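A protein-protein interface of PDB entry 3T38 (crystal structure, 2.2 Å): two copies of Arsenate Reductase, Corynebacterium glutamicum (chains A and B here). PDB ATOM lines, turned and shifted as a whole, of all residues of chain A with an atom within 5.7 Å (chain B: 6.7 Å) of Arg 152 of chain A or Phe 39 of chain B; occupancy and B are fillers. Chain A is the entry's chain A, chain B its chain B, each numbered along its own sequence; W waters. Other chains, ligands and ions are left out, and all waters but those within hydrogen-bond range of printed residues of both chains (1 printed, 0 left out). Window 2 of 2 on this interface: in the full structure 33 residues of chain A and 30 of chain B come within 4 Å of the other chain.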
ATOM      1  N   ALA A  69     -13.582   9.279  -4.891  1.00  0.00           N
ATOM      2  CA  ALA A  69     -14.219   8.083  -5.402  1.00  0.00           C
ATOM      3  C   ALA A  69     -13.924   6.877  -4.486  1.00  0.00           C
ATOM      4  O   ALA A  69     -14.861   6.197  -4.064  1.00  0.00           O
ATOM      5  CB  ALA A  69     -13.814   7.787  -6.832  1.00  0.00           C
ATOM      6  N   LEU A  70     -12.673   6.642  -4.123  1.00  0.00           N
ATOM      7  CA  LEU A  70     -12.362   5.501  -3.259  1.00  0.00           C
ATOM      8  C   LEU A  70     -12.998   5.575  -1.858  1.00  0.00           C
ATOM      9  O   LEU A  70     -13.443   4.565  -1.327  1.00  0.00           O
ATOM     10  CB  LEU A  70     -10.845   5.318  -3.134  1.00  0.00           C
ATOM     11  CG  LEU A  70     -10.286   4.069  -2.418  1.00  0.00           C
ATOM     12  CD1 LEU A  70     -10.748   2.773  -3.159  1.00  0.00           C
ATOM     13  CD2 LEU A  70      -8.767   4.126  -2.357  1.00  0.00           C
ATOM     14  N   ALA A  73     -16.621   4.570  -2.527  1.00  0.00           N
ATOM     15  CA  ALA A  73     -16.650   3.137  -2.777  1.00  0.00           C
ATOM     16  C   ALA A  73     -16.646   2.363  -1.467  1.00  0.00           C
ATOM     17  O   ALA A  73     -17.326   1.357  -1.340  1.00  0.00           O
ATOM     18  CB  ALA A  73     -15.460   2.728  -3.655  1.00  0.00           C
ATOM     19  N   ASP A 148      -9.902   1.872 -11.403  1.00  0.00           N
ATOM     20  CA  ASP A 148     -10.834   1.002 -10.713  1.00  0.00           C
ATOM     21  C   ASP A 148     -11.567   1.767  -9.634  1.00  0.00           C
ATOM     22  O   ASP A 148     -12.746   1.547  -9.449  1.00  0.00           O
ATOM     23  CB  ASP A 148     -10.054  -0.158 -10.035  1.00  0.00           C
ATOM     24  CG  ASP A 148     -10.971  -1.245  -9.499  1.00  0.00           C
ATOM     25  OD1 ASP A 148     -11.605  -1.935 -10.337  1.00  0.00           O
ATOM     26  OD2 ASP A 148     -11.003  -1.417  -8.270  1.00  0.00           O
ATOM     27  N   ASP A 149     -10.891   2.673  -8.919  1.00  0.00           N
ATOM     28  CA  ASP A 149     -11.563   3.362  -7.809  1.00  0.00           C
ATOM     29  C   ASP A 149     -12.877   4.019  -8.297  1.00  0.00           C
ATOM     30  O   ASP A 149     -13.893   3.928  -7.625  1.00  0.00           O
ATOM     31  CB  ASP A 149     -10.672   4.417  -7.158  1.00  0.00           C
ATOM     32  CG  ASP A 149      -9.788   5.122  -8.157  1.00  0.00           C
ATOM     33  OD1 ASP A 149     -10.194   5.386  -9.351  1.00  0.00           O
ATOM     34  OD2 ASP A 149      -8.623   5.314  -7.792  1.00  0.00           O
ATOM     35  N   VAL A 150     -12.862   4.659  -9.469  1.00  0.00           N
ATOM     36  CA  VAL A 150     -14.062   5.360  -9.944  1.00  0.00           C
ATOM     37  C   VAL A 150     -15.180   4.452 -10.430  1.00  0.00           C
ATOM     38  O   VAL A 150     -16.338   4.869 -10.401  1.00  0.00           O
ATOM     39  CB  VAL A 150     -13.767   6.511 -10.956  1.00  0.00           C
ATOM     40  CG1 VAL A 150     -12.701   7.453 -10.308  1.00  0.00           C
ATOM     41  CG2 VAL A 150     -13.281   5.968 -12.299  1.00  0.00           C
ATOM     42  N   ILE A 151     -14.838   3.223 -10.828  1.00  0.00           N
ATOM     43  CA  ILE A 151     -15.829   2.263 -11.145  1.00  0.00           C
ATOM     44  C   ILE A 151     -16.499   1.834  -9.862  1.00  0.00           C
ATOM     45  O   ILE A 151     -17.721   1.825  -9.774  1.00  0.00           O
ATOM     46  CB  ILE A 151     -15.260   1.049 -11.904  1.00  0.00           C
ATOM     47  CG1 ILE A 151     -14.637   1.464 -13.269  1.00  0.00           C
ATOM     48  CG2 ILE A 151     -16.386   0.015 -12.153  1.00  0.00           C
ATOM     49  CD1 ILE A 151     -13.637   0.324 -13.845  1.00  0.00           C
ATOM     50  N   ARG A 152     -15.712   1.530  -8.840  1.00  0.00           N
ATOM     51  CA  ARG A 152     -16.256   1.057  -7.536  1.00  0.00           C
ATOM     52  C   ARG A 152     -17.183   2.086  -6.891  1.00  0.00           C
ATOM     53  O   ARG A 152     -18.181   1.747  -6.207  1.00  0.00           O
ATOM     54  CB  ARG A 152     -15.137   0.732  -6.587  1.00  0.00           C
ATOM     55  CG  ARG A 152     -14.343  -0.528  -6.937  1.00  0.00           C
ATOM     56  CD  ARG A 152     -13.367  -0.892  -5.821  1.00  0.00           C
ATOM     57  NE  ARG A 152     -12.548  -2.074  -6.091  1.00  0.00           N
ATOM     58  CZ  ARG A 152     -12.710  -3.236  -5.470  1.00  0.00           C
ATOM     59  NH1 ARG A 152     -13.679  -3.404  -4.560  1.00  0.00           N
ATOM     60  NH2 ARG A 152     -11.933  -4.250  -5.785  1.00  0.00           N
ATOM     61  N   ALA A 153     -16.845   3.359  -7.091  1.00  0.00           N
ATOM     62  CA  ALA A 153     -17.647   4.401  -6.446  1.00  0.00           C
ATOM     63  C   ALA A 153     -18.985   4.525  -7.201  1.00  0.00           C
ATOM     64  O   ALA A 153     -19.909   5.017  -6.642  1.00  0.00           O
ATOM     65  CB  ALA A 153     -16.873   5.737  -6.477  1.00  0.00           C
ATOM     66  N   SER A 154     -19.040   4.170  -8.498  1.00  0.00           N
ATOM     67  CA  SER A 154     -20.115   4.593  -9.356  1.00  0.00           C
ATOM     68  C   SER A 154     -21.427   3.793  -9.081  1.00  0.00           C
ATOM     69  O   SER A 154     -21.373   2.589  -8.802  1.00  0.00           O
ATOM     70  CB  SER A 154     -19.668   4.468 -10.818  1.00  0.00           C
ATOM     71  OG  SER A 154     -18.657   5.425 -11.105  1.00  0.00           O
ATOM     72  N   TYR A 169     -18.753  -4.936 -11.658  1.00  0.00           N
ATOM     73  CA  TYR A 169     -19.100  -5.068 -10.226  1.00  0.00           C
ATOM     74  C   TYR A 169     -20.604  -5.126  -9.982  1.00  0.00           C
ATOM     75  O   TYR A 169     -21.357  -4.370 -10.597  1.00  0.00           O
ATOM     76  CB  TYR A 169     -18.494  -3.927  -9.366  1.00  0.00           C
ATOM     77  CG  TYR A 169     -16.983  -3.897  -9.303  1.00  0.00           C
ATOM     78  CD1 TYR A 169     -16.284  -4.813  -8.526  1.00  0.00           C
ATOM     79  CD2 TYR A 169     -16.260  -2.988 -10.048  1.00  0.00           C
ATOM     80  CE1 TYR A 169     -14.902  -4.805  -8.477  1.00  0.00           C
ATOM     81  CE2 TYR A 169     -14.860  -2.960 -10.002  1.00  0.00           C
ATOM     82  CZ  TYR A 169     -14.189  -3.870  -9.217  1.00  0.00           C
ATOM     83  OH  TYR A 169     -12.813  -3.865  -9.173  1.00  0.00           O
ATOM     84  N   LYS A 172     -24.670  -2.149  -9.148  1.00  0.00           N
ATOM     85  CA  LYS A 172     -24.527  -1.043 -10.069  1.00  0.00           C
ATOM     86  C   LYS A 172     -25.352  -1.202 -11.355  1.00  0.00           C
ATOM     87  O   LYS A 172     -25.524  -2.318 -11.846  1.00  0.00           O
ATOM     88  CB  LYS A 172     -23.052  -0.914 -10.494  1.00  0.00           C
ATOM     89  CG  LYS A 172     -22.054  -0.706  -9.383  1.00  0.00           C
ATOM     90  CD  LYS A 172     -20.610  -0.526  -9.900  1.00  0.00           C
ATOM     91  CE  LYS A 172     -19.633  -0.674  -8.672  1.00  0.00           C
ATOM     92  NZ  LYS A 172     -19.941   0.416  -7.746  1.00  0.00           N
ATOM     93  N   HIS B  10     -13.608 -11.711 -12.632  1.00  0.00           N
ATOM     94  CA  HIS B  10     -12.323 -11.985 -12.018  1.00  0.00           C
ATOM     95  C   HIS B  10     -12.183 -11.438 -10.608  1.00  0.00           C
ATOM     96  O   HIS B  10     -11.146 -11.521 -10.026  1.00  0.00           O
ATOM     97  CB  HIS B  10     -11.223 -11.439 -12.866  1.00  0.00           C
ATOM     98  CG  HIS B  10     -11.073 -12.133 -14.168  1.00  0.00           C
ATOM     99  ND1 HIS B  10     -10.842 -11.466 -15.342  1.00  0.00           N
ATOM    100  CD2 HIS B  10     -11.094 -13.442 -14.481  1.00  0.00           C
ATOM    101  CE1 HIS B  10     -10.736 -12.327 -16.325  1.00  0.00           C
ATOM    102  NE2 HIS B  10     -10.878 -13.534 -15.826  1.00  0.00           N
ATOM    103  N   THR B  11     -13.253 -10.896 -10.065  1.00  0.00           N
ATOM    104  CA  THR B  11     -13.225 -10.305  -8.739  1.00  0.00           C
ATOM    105  C   THR B  11     -12.680 -11.265  -7.717  1.00  0.00           C
ATOM    106  O   THR B  11     -11.762 -10.919  -6.980  1.00  0.00           O
ATOM    107  CB  THR B  11     -14.609  -9.820  -8.335  1.00  0.00           C
ATOM    108  OG1 THR B  11     -15.135  -9.057  -9.424  1.00  0.00           O
ATOM    109  CG2 THR B  11     -14.570  -8.964  -7.034  1.00  0.00           C
ATOM    110  N   ASN B  12     -13.222 -12.485  -7.694  1.00  0.00           N
ATOM    111  CA  ASN B  12     -12.807 -13.484  -6.704  1.00  0.00           C
ATOM    112  C   ASN B  12     -11.315 -13.809  -6.740  1.00  0.00           C
ATOM    113  O   ASN B  12     -10.675 -13.778  -5.692  1.00  0.00           O
ATOM    114  CB  ASN B  12     -13.673 -14.769  -6.765  1.00  0.00           C
ATOM    115  CG  ASN B  12     -15.142 -14.522  -6.353  1.00  0.00           C
ATOM    116  OD1 ASN B  12     -15.585 -13.364  -6.227  1.00  0.00           O
ATOM    117  ND2 ASN B  12     -15.906 -15.614  -6.171  1.00  0.00           N
ATOM    118  N   ILE B  13     -10.761 -14.095  -7.924  1.00  0.00           N
ATOM    119  CA  ILE B  13      -9.331 -14.430  -8.009  1.00  0.00           C
ATOM    120  C   ILE B  13      -8.443 -13.233  -7.688  1.00  0.00           C
ATOM    121  O   ILE B  13      -7.328 -13.392  -7.159  1.00  0.00           O
ATOM    122  CB  ILE B  13      -8.857 -15.015  -9.381  1.00  0.00           C
ATOM    123  CG1 ILE B  13      -9.115 -14.033 -10.529  1.00  0.00           C
ATOM    124  CG2 ILE B  13      -9.386 -16.435  -9.619  1.00  0.00           C
ATOM    125  CD1 ILE B  13      -9.589 -14.719 -11.836  1.00  0.00           C
ATOM    126  N   LEU B  14      -8.915 -12.043  -8.025  1.00  0.00           N
ATOM    127  CA  LEU B  14      -8.124 -10.874  -7.712  1.00  0.00           C
ATOM    128  C   LEU B  14      -8.085 -10.718  -6.194  1.00  0.00           C
ATOM    129  O   LEU B  14      -7.028 -10.427  -5.628  1.00  0.00           O
ATOM    130  CB  LEU B  14      -8.669  -9.621  -8.411  1.00  0.00           C
ATOM    131  CG  LEU B  14      -8.677  -9.607  -9.949  1.00  0.00           C
ATOM    132  CD1 LEU B  14      -9.552  -8.476 -10.430  1.00  0.00           C
ATOM    133  CD2 LEU B  14      -7.255  -9.484 -10.546  1.00  0.00           C
ATOM    134  N   ASN B  15      -9.236 -10.944  -5.550  1.00  0.00           N
ATOM    135  CA  ASN B  15      -9.358 -10.900  -4.090  1.00  0.00           C
ATOM    136  C   ASN B  15      -8.421 -11.925  -3.454  1.00  0.00           C
ATOM    137  O   ASN B  15      -7.636 -11.585  -2.569  1.00  0.00           O
ATOM    138  CB  ASN B  15     -10.806 -11.189  -3.655  1.00  0.00           C
ATOM    139  CG  ASN B  15     -11.678  -9.937  -3.585  1.00  0.00           C
ATOM    140  OD1 ASN B  15     -11.195  -8.810  -3.724  1.00  0.00           O
ATOM    141  ND2 ASN B  15     -12.981 -10.136  -3.337  1.00  0.00           N
ATOM    142  N   ALA B  18      -4.784 -10.747  -4.060  1.00  0.00           N
ATOM    143  CA  ALA B  18      -4.527  -9.692  -3.130  1.00  0.00           C
ATOM    144  C   ALA B  18      -4.232 -10.238  -1.750  1.00  0.00           C
ATOM    145  O   ALA B  18      -3.220  -9.858  -1.171  1.00  0.00           O
ATOM    146  CB  ALA B  18      -5.719  -8.769  -3.074  1.00  0.00           C
ATOM    147  N   ILE B  34      -1.830  -2.992  -1.050  1.00  0.00           N
ATOM    148  CA  ILE B  34      -1.805  -4.210  -1.828  1.00  0.00           C
ATOM    149  C   ILE B  34      -3.071  -4.411  -2.637  1.00  0.00           C
ATOM    150  O   ILE B  34      -2.959  -4.691  -3.839  1.00  0.00           O
ATOM    151  CB  ILE B  34      -1.576  -5.455  -0.929  1.00  0.00           C
ATOM    152  CG1 ILE B  34      -0.294  -5.308  -0.096  1.00  0.00           C
ATOM    153  CG2 ILE B  34      -1.542  -6.730  -1.776  1.00  0.00           C
ATOM    154  CD1 ILE B  34       0.968  -5.364  -0.872  1.00  0.00           C
ATOM    155  N   ASN B  35      -4.250  -4.279  -2.010  1.00  0.00           N
ATOM    156  CA  ASN B  35      -5.525  -4.365  -2.716  1.00  0.00           C
ATOM    157  C   ASN B  35      -5.530  -3.390  -3.860  1.00  0.00           C
ATOM    158  O   ASN B  35      -5.863  -3.761  -4.984  1.00  0.00           O
ATOM    159  CB  ASN B  35      -6.734  -4.013  -1.825  1.00  0.00           C
ATOM    160  CG  ASN B  35      -7.180  -5.167  -0.936  1.00  0.00           C
ATOM    161  OD1 ASN B  35      -7.104  -6.347  -1.331  1.00  0.00           O
ATOM    162  ND2 ASN B  35      -7.704  -4.830   0.272  1.00  0.00           N
ATOM    163  N   ARG B  36      -5.158  -2.138  -3.591  1.00  0.00           N
ATOM    164  CA  ARG B  36      -5.257  -1.164  -4.651  1.00  0.00           C
ATOM    165  C   ARG B  36      -4.349  -1.529  -5.816  1.00  0.00           C
ATOM    166  O   ARG B  36      -4.821  -1.562  -6.935  1.00  0.00           O
ATOM    167  CB  ARG B  36      -5.079   0.263  -4.174  1.00  0.00           C
ATOM    168  CG  ARG B  36      -6.209   0.747  -3.260  1.00  0.00           C
ATOM    169  CD  ARG B  36      -7.444   1.121  -4.039  1.00  0.00           C
ATOM    170  NE  ARG B  36      -8.336   0.000  -4.180  1.00  0.00           N
ATOM    171  CZ  ARG B  36      -9.098  -0.267  -5.238  1.00  0.00           C
ATOM    172  NH1 ARG B  36      -9.103   0.497  -6.310  1.00  0.00           N
ATOM    173  NH2 ARG B  36      -9.870  -1.348  -5.187  1.00  0.00           N
ATOM    174  N   TYR B  37      -3.084  -1.882  -5.534  1.00  0.00           N
ATOM    175  CA  TYR B  37      -2.141  -2.373  -6.553  1.00  0.00           C
ATOM    176  C   TYR B  37      -2.694  -3.430  -7.515  1.00  0.00           C
ATOM    177  O   TYR B  37      -2.535  -3.333  -8.731  1.00  0.00           O
ATOM    178  CB  TYR B  37      -0.846  -2.882  -5.904  1.00  0.00           C
ATOM    179  CG  TYR B  37       0.200  -1.808  -5.970  1.00  0.00           C
ATOM    180  CD1 TYR B  37       1.027  -1.717  -7.074  1.00  0.00           C
ATOM    181  CD2 TYR B  37       0.292  -0.829  -4.994  1.00  0.00           C
ATOM    182  CE1 TYR B  37       1.955  -0.692  -7.204  1.00  0.00           C
ATOM    183  CE2 TYR B  37       1.227   0.209  -5.104  1.00  0.00           C
ATOM    184  CZ  TYR B  37       2.064   0.263  -6.215  1.00  0.00           C
ATOM    185  OH  TYR B  37       3.017   1.271  -6.392  1.00  0.00           O
ATOM    186  N   ILE B  38      -3.382  -4.413  -6.953  1.00  0.00           N
ATOM    187  CA  ILE B  38      -3.886  -5.502  -7.747  1.00  0.00           C
ATOM    188  C   ILE B  38      -5.090  -5.085  -8.621  1.00  0.00           C
ATOM    189  O   ILE B  38      -5.112  -5.313  -9.859  1.00  0.00           O
ATOM    190  CB  ILE B  38      -4.064  -6.755  -6.886  1.00  0.00           C
ATOM    191  CG1 ILE B  38      -3.711  -7.943  -7.727  1.00  0.00           C
ATOM    192  CG2 ILE B  38      -5.466  -6.939  -6.425  1.00  0.00           C
ATOM    193  CD1 ILE B  38      -4.807  -8.244  -8.704  1.00  0.00           C
ATOM    194  N   PHE B  39      -6.044  -4.400  -8.013  1.00  0.00           N
ATOM    195  CA  PHE B  39      -7.193  -3.951  -8.786  1.00  0.00           C
ATOM    196  C   PHE B  39      -6.861  -2.882  -9.834  1.00  0.00           C
ATOM    197  O   PHE B  39      -7.349  -2.960 -10.966  1.00  0.00           O
ATOM    198  CB  PHE B  39      -8.329  -3.568  -7.853  1.00  0.00           C
ATOM    199  CG  PHE B  39      -8.999  -4.762  -7.258  1.00  0.00           C
ATOM    200  CD1 PHE B  39      -8.664  -5.200  -5.977  1.00  0.00           C
ATOM    201  CD2 PHE B  39      -9.943  -5.481  -8.005  1.00  0.00           C
ATOM    202  CE1 PHE B  39      -9.260  -6.314  -5.423  1.00  0.00           C
ATOM    203  CE2 PHE B  39     -10.563  -6.580  -7.469  1.00  0.00           C
ATOM    204  CZ  PHE B  39     -10.204  -7.017  -6.163  1.00  0.00           C
ATOM    205  N   GLU B  40      -5.977  -1.938  -9.498  1.00  0.00           N
ATOM    206  CA  GLU B  40      -5.597  -0.898 -10.468  1.00  0.00           C
ATOM    207  C   GLU B  40      -4.763  -1.436 -11.638  1.00  0.00           C
ATOM    208  O   GLU B  40      -5.007  -1.062 -12.793  1.00  0.00           O
ATOM    209  CB  GLU B  40      -4.933   0.310  -9.766  1.00  0.00           C
ATOM    210  CG  GLU B  40      -5.837   1.064  -8.710  1.00  0.00           C
ATOM    211  CD  GLU B  40      -7.047   1.834  -9.308  1.00  0.00           C
ATOM    212  OE1 GLU B  40      -7.236   1.848 -10.552  1.00  0.00           O
ATOM    213  OE2 GLU B  40      -7.830   2.447  -8.501  1.00  0.00           O
ATOM    214  N   SER B  41      -3.865  -2.406 -11.343  1.00  0.00           N
ATOM    215  CA  SER B  41      -3.034  -3.040 -12.368  1.00  0.00           C
ATOM    216  C   SER B  41      -3.903  -3.806 -13.331  1.00  0.00           C
ATOM    217  O   SER B  41      -3.662  -3.814 -14.558  1.00  0.00           O
ATOM    218  CB  SER B  41      -2.002  -3.989 -11.726  1.00  0.00           C
ATOM    219  OG  SER B  41      -1.159  -3.269 -10.812  1.00  0.00           O
ATOM    220  N   TYR B  42      -4.900  -4.476 -12.768  1.00  0.00           N
ATOM    221  CA  TYR B  42      -5.900  -5.199 -13.552  1.00  0.00           C
ATOM    222  C   TYR B  42      -6.602  -4.254 -14.528  1.00  0.00           C
ATOM    223  O   TYR B  42      -6.609  -4.511 -15.726  1.00  0.00           O
ATOM    224  CB  TYR B  42      -6.893  -5.941 -12.636  1.00  0.00           C
ATOM    225  CG  TYR B  42      -7.939  -6.742 -13.378  1.00  0.00           C
ATOM    226  CD1 TYR B  42      -9.153  -6.172 -13.726  1.00  0.00           C
ATOM    227  CD2 TYR B  42      -7.703  -8.056 -13.763  1.00  0.00           C
ATOM    228  CE1 TYR B  42     -10.168  -6.925 -14.413  1.00  0.00           C
ATOM    229  CE2 TYR B  42      -8.671  -8.778 -14.454  1.00  0.00           C
ATOM    230  CZ  TYR B  42      -9.892  -8.205 -14.766  1.00  0.00           C
ATOM    231  OH  TYR B  42     -10.800  -8.917 -15.479  1.00  0.00           O
ATOM    232  N   VAL B  43      -7.182  -3.174 -14.017  1.00  0.00           N
ATOM    233  CA  VAL B  43      -7.906  -2.226 -14.861  1.00  0.00           C
ATOM    234  C   VAL B  43      -6.970  -1.536 -15.814  1.00  0.00           C
ATOM    235  O   VAL B  43      -7.305  -1.264 -16.979  1.00  0.00           O
ATOM    236  CB  VAL B  43      -8.742  -1.227 -14.050  1.00  0.00           C
ATOM    237  CG1 VAL B  43      -9.248  -0.077 -14.891  1.00  0.00           C
ATOM    238  CG2 VAL B  43     -10.005  -1.916 -13.624  1.00  0.00           C
ATOM    239  N   SER B  44      -5.759  -1.313 -15.357  1.00  0.00           N
ATOM    240  CA  SER B  44      -4.811  -0.595 -16.152  1.00  0.00           C
ATOM    241  C   SER B  44      -4.453  -1.378 -17.403  1.00  0.00           C
ATOM    242  O   SER B  44      -4.334  -0.806 -18.455  1.00  0.00           O
ATOM    243  CB  SER B  44      -3.540  -0.410 -15.345  1.00  0.00           C
ATOM    244  OG  SER B  44      -2.926   0.748 -15.777  1.00  0.00           O
ATOM    245  N   ALA B  59      -2.190  -9.315 -14.673  1.00  0.00           N
ATOM    246  CA  ALA B  59      -2.369  -8.332 -13.568  1.00  0.00           C
ATOM    247  C   ALA B  59      -1.528  -8.663 -12.337  1.00  0.00           C
ATOM    248  O   ALA B  59      -0.967  -7.769 -11.726  1.00  0.00           O
ATOM    249  CB  ALA B  59      -3.857  -8.140 -13.179  1.00  0.00           C
ATOM    250  N   ALA B  63       1.484  -6.341 -10.943  1.00  0.00           N
ATOM    251  CA  ALA B  63       1.397  -5.838  -9.567  1.00  0.00           C
ATOM    252  C   ALA B  63       2.597  -6.282  -8.712  1.00  0.00           C
ATOM    253  O   ALA B  63       3.151  -5.488  -7.946  1.00  0.00           O
ATOM    254  CB  ALA B  63       0.030  -6.251  -8.871  1.00  0.00           C
HETATM  255  O   HOH W   1     -12.139  -5.739  -3.113  1.00  0.00           O
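No position is printed for both chains.
Of the 12 printed residues of chain A, 5 touch a printed residue of chain B.
Printed residues of chain A that touch a printed residue of chain B: Leu 70, Asp 148, Asp 149, Arg 152 and Tyr 169.
Among the printed residues, Asp or Glu carboxylates within 4 Å of a Lys or Arg side-chain nitrogen of the other chain: Asp 148 of chain A with Arg 36 of chain B.
Arg 36 of chain B touches Leu 70 of chain A (CD to CD2, 3.7 Å).
CB of Phe 39 of chain B touches OD2 of Asp 148 of chain A, 3.5 Å away.
Val 43 of chain B touches Asp 148 of chain A.
Asp 149 of chain A touches Arg 36 of chain B.
Arg 152 of chain A touches Phe 39 of chain B (NH2 to CE2, 3.2 Å).
Phe 39 of chain B touches Tyr 169 of chain A.
Water W1 lies within hydrogen-bond range of the guanidinium group (NH2) of Arg 152 of chain A (3.1 Å) and the side-chain amide oxygen (OD1) of Asn 15 of chain B (3.3 Å).
N of Asp 148 of chain A is in hydrogen-bond range of OE1 of Glu 40 of chain B.
N of Asp 149 of chain A is in hydrogen-bond range of OE2 of Glu 40 of chain B (3.1 Å).
NH2 of Arg 36 of chain B lies close to NE of Arg 152 of chain A, 2.9 Å away.
OD2 of Asp 148 of chain A lies within salt-bridge range of NH2 of Arg 36 of chain B, 3.3 Å away.
NH1 of Arg 36 of chain B is in salt-bridge range of OE2 of Glu 40 of chain B, 3.2 Å away.
OD1 of Asp 148 of chain A is in hydrogen-bond range of OH of Tyr 169 of chain A (2.6 Å).
The backbone carbonyl oxygen (O) of Arg 152 of chain A sits at hydrogen-bond distance from the side-chain amino group (NZ) of Lys 172 of chain A.
The side-chain carboxylate (OD2) of Asp 148 of chain A lies within salt-bridge range of the guanidinium group (NE) of Arg 152 of chain A.
Arg 152 of chain A touches just these residues of chain B: Arg 36 and Phe 39.
Of the printed residues of chain A, Arg 36 of chain B touches Leu 70 (3.7 Å), Asp 148 (3.3 Å), Asp 149 (3.8 Å) and Arg 152 (2.9 Å).
Printed residues of chain A within 4 Å of Val 43 of chain B: Asp 148 (3.7 Å).
Of the printed residues of chain B, Asp 149 of chain A touches Arg 36 and Glu 40.
The nearest residue of chain B that does not touch Arg 152 of chain A is Asn 15 of chain B (5.1 Å).
The nearest printed residue of chain A that does not touch Phe 39 of chain B is Asp 149 of chain A (6.8 Å).
The nearest printed residue of chain B that does not touch Leu 70 of chain A is Glu 40 of chain B (6.1 Å).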
